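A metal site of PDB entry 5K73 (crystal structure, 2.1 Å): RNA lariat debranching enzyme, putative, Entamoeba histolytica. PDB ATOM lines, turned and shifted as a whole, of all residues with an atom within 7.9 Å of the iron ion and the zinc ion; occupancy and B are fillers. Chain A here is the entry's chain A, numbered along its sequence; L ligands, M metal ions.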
ATOM      1  N   GLY A  15     -31.064   8.723  -9.930  1.00  0.00           N
ATOM      2  CA  GLY A  15     -30.654   9.033 -11.285  1.00  0.00           C
ATOM      3  C   GLY A  15     -29.906  10.344 -11.394  1.00  0.00           C
ATOM      4  O   GLY A  15     -28.773  10.456 -10.921  1.00  0.00           O
ATOM      5  N   CYS A  16     -30.517  11.345 -12.018  1.00  0.00           N
ATOM      6  CA  CYS A  16     -29.909  12.660 -12.191  1.00  0.00           C
ATOM      7  C   CYS A  16     -30.346  13.588 -11.064  1.00  0.00           C
ATOM      8  O   CYS A  16     -31.540  13.677 -10.755  1.00  0.00           O
ATOM      9  CB  CYS A  16     -30.289  13.254 -13.537  1.00  0.00           C
ATOM     10  SG  CYS A  16     -29.735  12.313 -14.977  1.00  0.00           S
ATOM     11  N   VAL A  17     -29.385  14.270 -10.450  1.00  0.00           N
ATOM     12  CA  VAL A  17     -29.682  15.224  -9.388  1.00  0.00           C
ATOM     13  C   VAL A  17     -29.902  16.623  -9.955  1.00  0.00           C
ATOM     14  O   VAL A  17     -30.868  17.298  -9.609  1.00  0.00           O
ATOM     15  CB  VAL A  17     -28.564  15.212  -8.329  1.00  0.00           C
ATOM     16  CG1 VAL A  17     -28.682  16.426  -7.422  1.00  0.00           C
ATOM     17  CG2 VAL A  17     -28.643  13.939  -7.514  1.00  0.00           C
ATOM     18  N   HIS A  18     -28.998  17.064 -10.836  1.00  0.00           N
ATOM     19  CA  HIS A  18     -29.072  18.387 -11.464  1.00  0.00           C
ATOM     20  C   HIS A  18     -29.131  19.503 -10.417  1.00  0.00           C
ATOM     21  O   HIS A  18     -29.875  20.475 -10.562  1.00  0.00           O
ATOM     22  CB  HIS A  18     -30.249  18.484 -12.424  1.00  0.00           C
ATOM     23  CG  HIS A  18     -30.056  17.707 -13.692  1.00  0.00           C
ATOM     24  ND1 HIS A  18     -29.155  18.077 -14.662  1.00  0.00           N
ATOM     25  CD2 HIS A  18     -30.647  16.577 -14.140  1.00  0.00           C
ATOM     26  CE1 HIS A  18     -29.189  17.211 -15.659  1.00  0.00           C
ATOM     27  NE2 HIS A  18     -30.091  16.289 -15.368  1.00  0.00           N
ATOM     28  N   THR A  45     -26.167   8.458  -9.978  1.00  0.00           N
ATOM     29  CA  THR A  45     -25.583   8.147 -11.282  1.00  0.00           C
ATOM     30  C   THR A  45     -25.017   9.349 -12.012  1.00  0.00           C
ATOM     31  O   THR A  45     -24.481   9.174 -13.117  1.00  0.00           O
ATOM     32  CB  THR A  45     -26.614   7.451 -12.171  1.00  0.00           C
ATOM     33  OG1 THR A  45     -27.759   8.298 -12.336  1.00  0.00           O
ATOM     34  CG2 THR A  45     -27.053   6.128 -11.559  1.00  0.00           C
ATOM     35  N   GLY A  46     -25.112  10.552 -11.473  1.00  0.00           N
ATOM     36  CA  GLY A  46     -24.391  11.667 -12.045  1.00  0.00           C
ATOM     37  C   GLY A  46     -25.242  12.919 -12.176  1.00  0.00           C
ATOM     38  O   GLY A  46     -26.345  12.990 -11.637  1.00  0.00           O
ATOM     39  N   ASP A  47     -24.696  13.877 -12.908  1.00  0.00           N
ATOM     40  CA  ASP A  47     -25.246  15.232 -13.020  1.00  0.00           C
ATOM     41  C   ASP A  47     -25.387  15.871 -11.640  1.00  0.00           C
ATOM     42  O   ASP A  47     -26.461  16.327 -11.227  1.00  0.00           O
ATOM     43  CB  ASP A  47     -26.571  15.235 -13.786  1.00  0.00           C
ATOM     44  CG  ASP A  47     -26.376  15.001 -15.272  1.00  0.00           C
ATOM     45  OD1 ASP A  47     -25.214  15.066 -15.737  1.00  0.00           O
ATOM     46  OD2 ASP A  47     -27.374  14.755 -15.983  1.00  0.00           O
ATOM     47  N   GLN A  49     -23.480  18.538 -10.458  1.00  0.00           N
ATOM     48  CA  GLN A  49     -23.286  19.988 -10.510  1.00  0.00           C
ATOM     49  C   GLN A  49     -22.720  20.513  -9.185  1.00  0.00           C
ATOM     50  O   GLN A  49     -23.310  21.354  -8.509  1.00  0.00           O
ATOM     51  CB  GLN A  49     -24.594  20.703 -10.854  1.00  0.00           C
ATOM     52  CG  GLN A  49     -25.264  20.205 -12.125  1.00  0.00           C
ATOM     53  CD  GLN A  49     -26.477  21.024 -12.513  1.00  0.00           C
ATOM     54  OE1 GLN A  49     -26.702  22.099 -11.960  1.00  0.00           O
ATOM     55  NE2 GLN A  49     -27.249  20.531 -13.461  1.00  0.00           N
ATOM     56  N   GLY A  90     -19.638  11.121 -12.138  1.00  0.00           N
ATOM     57  CA  GLY A  90     -19.897  12.312 -12.907  1.00  0.00           C
ATOM     58  C   GLY A  90     -20.781  12.046 -14.113  1.00  0.00           C
ATOM     59  O   GLY A  90     -20.748  10.960 -14.697  1.00  0.00           O
ATOM     60  N   GLY A  91     -21.576  13.047 -14.476  1.00  0.00           N
ATOM     61  CA  GLY A  91     -22.396  12.959 -15.666  1.00  0.00           C
ATOM     62  C   GLY A  91     -21.919  13.896 -16.749  1.00  0.00           C
ATOM     63  O   GLY A  91     -20.714  14.022 -16.980  1.00  0.00           O
ATOM     64  N   ASN A  92     -22.857  14.567 -17.434  1.00  0.00           N
ATOM     65  CA  ASN A  92     -22.519  15.579 -18.422  1.00  0.00           C
ATOM     66  C   ASN A  92     -22.816  16.996 -17.949  1.00  0.00           C
ATOM     67  O   ASN A  92     -22.387  17.948 -18.614  1.00  0.00           O
ATOM     68  CB  ASN A  92     -23.251  15.304 -19.748  1.00  0.00           C
ATOM     69  CG  ASN A  92     -24.758  15.223 -19.570  1.00  0.00           C
ATOM     70  OD1 ASN A  92     -25.278  14.231 -19.054  1.00  0.00           O
ATOM     71  ND2 ASN A  92     -25.467  16.256 -20.012  1.00  0.00           N
ATOM     72  N   HIS A  93     -23.516  17.155 -16.840  1.00  0.00           N
ATOM     73  CA  HIS A  93     -23.753  18.465 -16.215  1.00  0.00           C
ATOM     74  C   HIS A  93     -23.004  18.475 -14.886  1.00  0.00           C
ATOM     75  O   HIS A  93     -23.543  18.067 -13.851  1.00  0.00           O
ATOM     76  CB  HIS A  93     -25.244  18.723 -16.027  1.00  0.00           C
ATOM     77  CG  HIS A  93     -25.970  18.994 -17.302  1.00  0.00           C
ATOM     78  ND1 HIS A  93     -27.319  19.280 -17.337  1.00  0.00           N
ATOM     79  CD2 HIS A  93     -25.546  19.037 -18.582  1.00  0.00           C
ATOM     80  CE1 HIS A  93     -27.691  19.481 -18.587  1.00  0.00           C
ATOM     81  NE2 HIS A  93     -26.637  19.337 -19.359  1.00  0.00           N
ATOM     82  N   GLU A  94     -21.758  18.923 -14.917  1.00  0.00           N
ATOM     83  CA  GLU A  94     -20.893  18.892 -13.744  1.00  0.00           C
ATOM     84  C   GLU A  94     -20.020  20.140 -13.706  1.00  0.00           C
ATOM     85  O   GLU A  94     -19.796  20.805 -14.722  1.00  0.00           O
ATOM     86  CB  GLU A  94     -19.973  17.653 -13.747  1.00  0.00           C
ATOM     87  CG  GLU A  94     -20.681  16.317 -13.938  1.00  0.00           C
ATOM     88  CD  GLU A  94     -21.429  15.853 -12.698  1.00  0.00           C
ATOM     89  OE1 GLU A  94     -21.362  16.546 -11.658  1.00  0.00           O
ATOM     90  OE2 GLU A  94     -22.075  14.796 -12.771  1.00  0.00           O
ATOM     91  N   GLY A 133     -19.020  10.078 -16.786  1.00  0.00           N
ATOM     92  CA  GLY A 133     -19.071  10.700 -18.101  1.00  0.00           C
ATOM     93  C   GLY A 133     -20.082  10.078 -19.045  1.00  0.00           C
ATOM     94  O   GLY A 133     -20.741   9.068 -18.752  1.00  0.00           O
ATOM     95  N   ILE A 134     -20.200  10.704 -20.213  1.00  0.00           N
ATOM     96  CA  ILE A 134     -21.005  10.186 -21.309  1.00  0.00           C
ATOM     97  C   ILE A 134     -20.091   9.999 -22.509  1.00  0.00           C
ATOM     98  O   ILE A 134     -19.010  10.575 -22.598  1.00  0.00           O
ATOM     99  CB  ILE A 134     -22.197  11.094 -21.669  1.00  0.00           C
ATOM    100  CG1 ILE A 134     -21.714  12.447 -22.195  1.00  0.00           C
ATOM    101  CG2 ILE A 134     -23.109  11.273 -20.458  1.00  0.00           C
ATOM    102  CD1 ILE A 134     -22.825  13.296 -22.782  1.00  0.00           C
ATOM    103  N   HIS A 182     -23.319   6.798 -16.169  1.00  0.00           N
ATOM    104  CA  HIS A 182     -24.299   7.850 -16.358  1.00  0.00           C
ATOM    105  C   HIS A 182     -25.215   7.548 -17.541  1.00  0.00           C
ATOM    106  O   HIS A 182     -26.429   7.374 -17.363  1.00  0.00           O
ATOM    107  CB  HIS A 182     -23.620   9.213 -16.543  1.00  0.00           C
ATOM    108  CG  HIS A 182     -24.583  10.358 -16.487  1.00  0.00           C
ATOM    109  ND1 HIS A 182     -25.337  10.640 -15.365  1.00  0.00           N
ATOM    110  CD2 HIS A 182     -24.957  11.264 -17.423  1.00  0.00           C
ATOM    111  CE1 HIS A 182     -26.103  11.684 -15.604  1.00  0.00           C
ATOM    112  NE2 HIS A 182     -25.901  12.078 -16.844  1.00  0.00           N
ATOM    113  N   ASP A 183     -24.665   7.480 -18.746  1.00  0.00           N
ATOM    114  CA  ASP A 183     -25.467   7.032 -19.870  1.00  0.00           C
ATOM    115  C   ASP A 183     -25.511   5.501 -19.893  1.00  0.00           C
ATOM    116  O   ASP A 183     -24.710   4.810 -19.255  1.00  0.00           O
ATOM    117  CB  ASP A 183     -24.917   7.583 -21.191  1.00  0.00           C
ATOM    118  CG  ASP A 183     -23.439   7.333 -21.371  1.00  0.00           C
ATOM    119  OD1 ASP A 183     -22.753   6.962 -20.396  1.00  0.00           O
ATOM    120  OD2 ASP A 183     -22.943   7.519 -22.503  1.00  0.00           O
ATOM    121  N   GLY A 231     -28.419   6.603 -15.462  1.00  0.00           N
ATOM    122  CA  GLY A 231     -29.389   7.689 -15.476  1.00  0.00           C
ATOM    123  C   GLY A 231     -29.459   8.378 -16.828  1.00  0.00           C
ATOM    124  O   GLY A 231     -29.721   7.731 -17.839  1.00  0.00           O
ATOM    125  N   HIS A 232     -29.252   9.692 -16.831  1.00  0.00           N
ATOM    126  CA  HIS A 232     -29.073  10.491 -18.042  1.00  0.00           C
ATOM    127  C   HIS A 232     -30.346  10.674 -18.860  1.00  0.00           C
ATOM    128  O   HIS A 232     -30.677  11.799 -19.249  1.00  0.00           O
ATOM    129  CB  HIS A 232     -27.968   9.895 -18.920  1.00  0.00           C
ATOM    130  CG  HIS A 232     -27.596  10.730 -20.099  1.00  0.00           C
ATOM    131  ND1 HIS A 232     -27.095  12.010 -19.979  1.00  0.00           N
ATOM    132  CD2 HIS A 232     -27.654  10.471 -21.431  1.00  0.00           C
ATOM    133  CE1 HIS A 232     -26.850  12.498 -21.184  1.00  0.00           C
ATOM    134  NE2 HIS A 232     -27.183  11.589 -22.076  1.00  0.00           N
ATOM    135  N   MET A 233     -31.082   9.589 -19.118  1.00  0.00           N
ATOM    136  CA  MET A 233     -32.182   9.615 -20.080  1.00  0.00           C
ATOM    137  C   MET A 233     -33.490  10.127 -19.491  1.00  0.00           C
ATOM    138  O   MET A 233     -34.479  10.212 -20.232  1.00  0.00           O
ATOM    139  CB  MET A 233     -32.388   8.224 -20.676  1.00  0.00           C
ATOM    140  CG  MET A 233     -31.135   7.641 -21.328  1.00  0.00           C
ATOM    141  SD  MET A 233     -30.582   8.533 -22.795  1.00  0.00           S
ATOM    142  CE  MET A 233     -31.748   7.948 -24.017  1.00  0.00           C
ATOM    143  N   HIS A 234     -33.538  10.455 -18.198  1.00  0.00           N
ATOM    144  CA  HIS A 234     -34.700  11.065 -17.568  1.00  0.00           C
ATOM    145  C   HIS A 234     -35.948  10.190 -17.702  1.00  0.00           C
ATOM    146  O   HIS A 234     -37.052  10.674 -17.958  1.00  0.00           O
ATOM    147  CB  HIS A 234     -34.975  12.465 -18.125  1.00  0.00           C
ATOM    148  CG  HIS A 234     -33.836  13.418 -17.922  1.00  0.00           C
ATOM    149  ND1 HIS A 234     -33.770  14.640 -18.560  1.00  0.00           N
ATOM    150  CD2 HIS A 234     -32.727  13.330 -17.150  1.00  0.00           C
ATOM    151  CE1 HIS A 234     -32.659  15.269 -18.195  1.00  0.00           C
ATOM    152  NE2 HIS A 234     -32.010  14.497 -17.345  1.00  0.00           N
ATOM    153  N   LEU A 249     -32.774   5.262 -14.128  1.00  0.00           N
ATOM    154  CA  LEU A 249     -33.516   6.152 -13.266  1.00  0.00           C
ATOM    155  C   LEU A 249     -33.642   7.529 -13.908  1.00  0.00           C
ATOM    156  O   LEU A 249     -32.835   7.916 -14.761  1.00  0.00           O
ATOM    157  CB  LEU A 249     -32.850   6.273 -11.885  1.00  0.00           C
ATOM    158  CG  LEU A 249     -32.518   4.959 -11.183  1.00  0.00           C
ATOM    159  CD1 LEU A 249     -31.552   5.179 -10.034  1.00  0.00           C
ATOM    160  CD2 LEU A 249     -33.795   4.288 -10.682  1.00  0.00           C
ATOM    161  N   GLY A 250     -34.657   8.274 -13.476  1.00  0.00           N
ATOM    162  CA  GLY A 250     -34.928   9.600 -14.000  1.00  0.00           C
ATOM    163  C   GLY A 250     -34.204  10.693 -13.236  1.00  0.00           C
ATOM    164  O   GLY A 250     -33.206  10.458 -12.547  1.00  0.00           O
ATOM    165  N   LYS A 251     -34.703  11.916 -13.365  1.00  0.00           N
ATOM    166  CA  LYS A 251     -34.097  13.085 -12.749  1.00  0.00           C
ATOM    167  C   LYS A 251     -34.894  13.525 -11.529  1.00  0.00           C
ATOM    168  O   LYS A 251     -36.123  13.383 -11.477  1.00  0.00           O
ATOM    169  CB  LYS A 251     -33.998  14.238 -13.763  1.00  0.00           C
ATOM    170  CG  LYS A 251     -35.343  14.720 -14.293  1.00  0.00           C
ATOM    171  CD  LYS A 251     -35.175  15.714 -15.427  1.00  0.00           C
ATOM    172  CE  LYS A 251     -34.434  16.968 -14.992  1.00  0.00           C
ATOM    173  NZ  LYS A 251     -34.304  17.946 -16.097  1.00  0.00           N
ATOM    174  N   ILE A 252     -34.172  14.060 -10.542  1.00  0.00           N
ATOM    175  CA  ILE A 252     -34.810  14.521  -9.314  1.00  0.00           C
ATOM    176  C   ILE A 252     -35.872  15.561  -9.642  1.00  0.00           C
ATOM    177  O   ILE A 252     -35.669  16.452 -10.485  1.00  0.00           O
ATOM    178  CB  ILE A 252     -33.754  15.085  -8.349  1.00  0.00           C
ATOM    179  CG1 ILE A 252     -32.921  13.948  -7.755  1.00  0.00           C
ATOM    180  CG2 ILE A 252     -34.404  15.891  -7.235  1.00  0.00           C
ATOM    181  CD1 ILE A 252     -33.723  12.990  -6.885  1.00  0.00           C
HETATM  182  O1  LIG L   1     -29.555  14.415 -18.488  1.00  0.00           O
HETATM  183 FE    FE M   1     -27.054  13.501 -17.992  1.00  0.00          FE
HETATM  184 ZN    ZN M   2     -29.890  14.254 -16.394  1.00  0.00          ZN
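The iron ion is bound by NE2 of His 182 (2.2 Å), OD1 of Asn 92 (2.2 Å), OD2 of Asp 47 (2.4 Å) and ND1 of His 232 (2.5 Å). Slightly farther from the iron ion lies an oxygen (O1) of the ligand (2.7 Å).
Within 4 Å of the zinc ion: Cys 16, His 18, Asp 47, His 232 and His 234.
The backbone NH (N) of His 93 is in hydrogen-bond range of the side-chain carboxylate (OD1) of Asp 47, 2.9 Å away. The backbone carbonyl oxygen (O) of Thr 45 lies within hydrogen-bond range of a ring nitrogen (ND1) of His 182 (2.8 Å). N of Asp 47 is in hydrogen-bond range of OE2 of Glu 94 (2.8 Å). ND1 of His 18 lies within hydrogen-bond range of NE2 of Gln 49. The backbone NH (N) of Gly 231 sits at hydrogen-bond distance from the backbone carbonyl oxygen (O) of His 182. N of Cys 16 sits at hydrogen-bond distance from O of Gly 250, at 2.9 Å. ND1 of His 93 lies close to ND1 of His 18 (3.5 Å). NE2 of His 93 sits close to ND2 of Asn 92 (3.4 Å).
The zinc ion is bound by O1 of the ligand (2.1 Å), NE2 of His 18 (2.3 Å), NE2 of His 234 (2.3 Å), SG of Cys 16 (2.4 Å) and OD2 of Asp 47 (2.6 Å).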
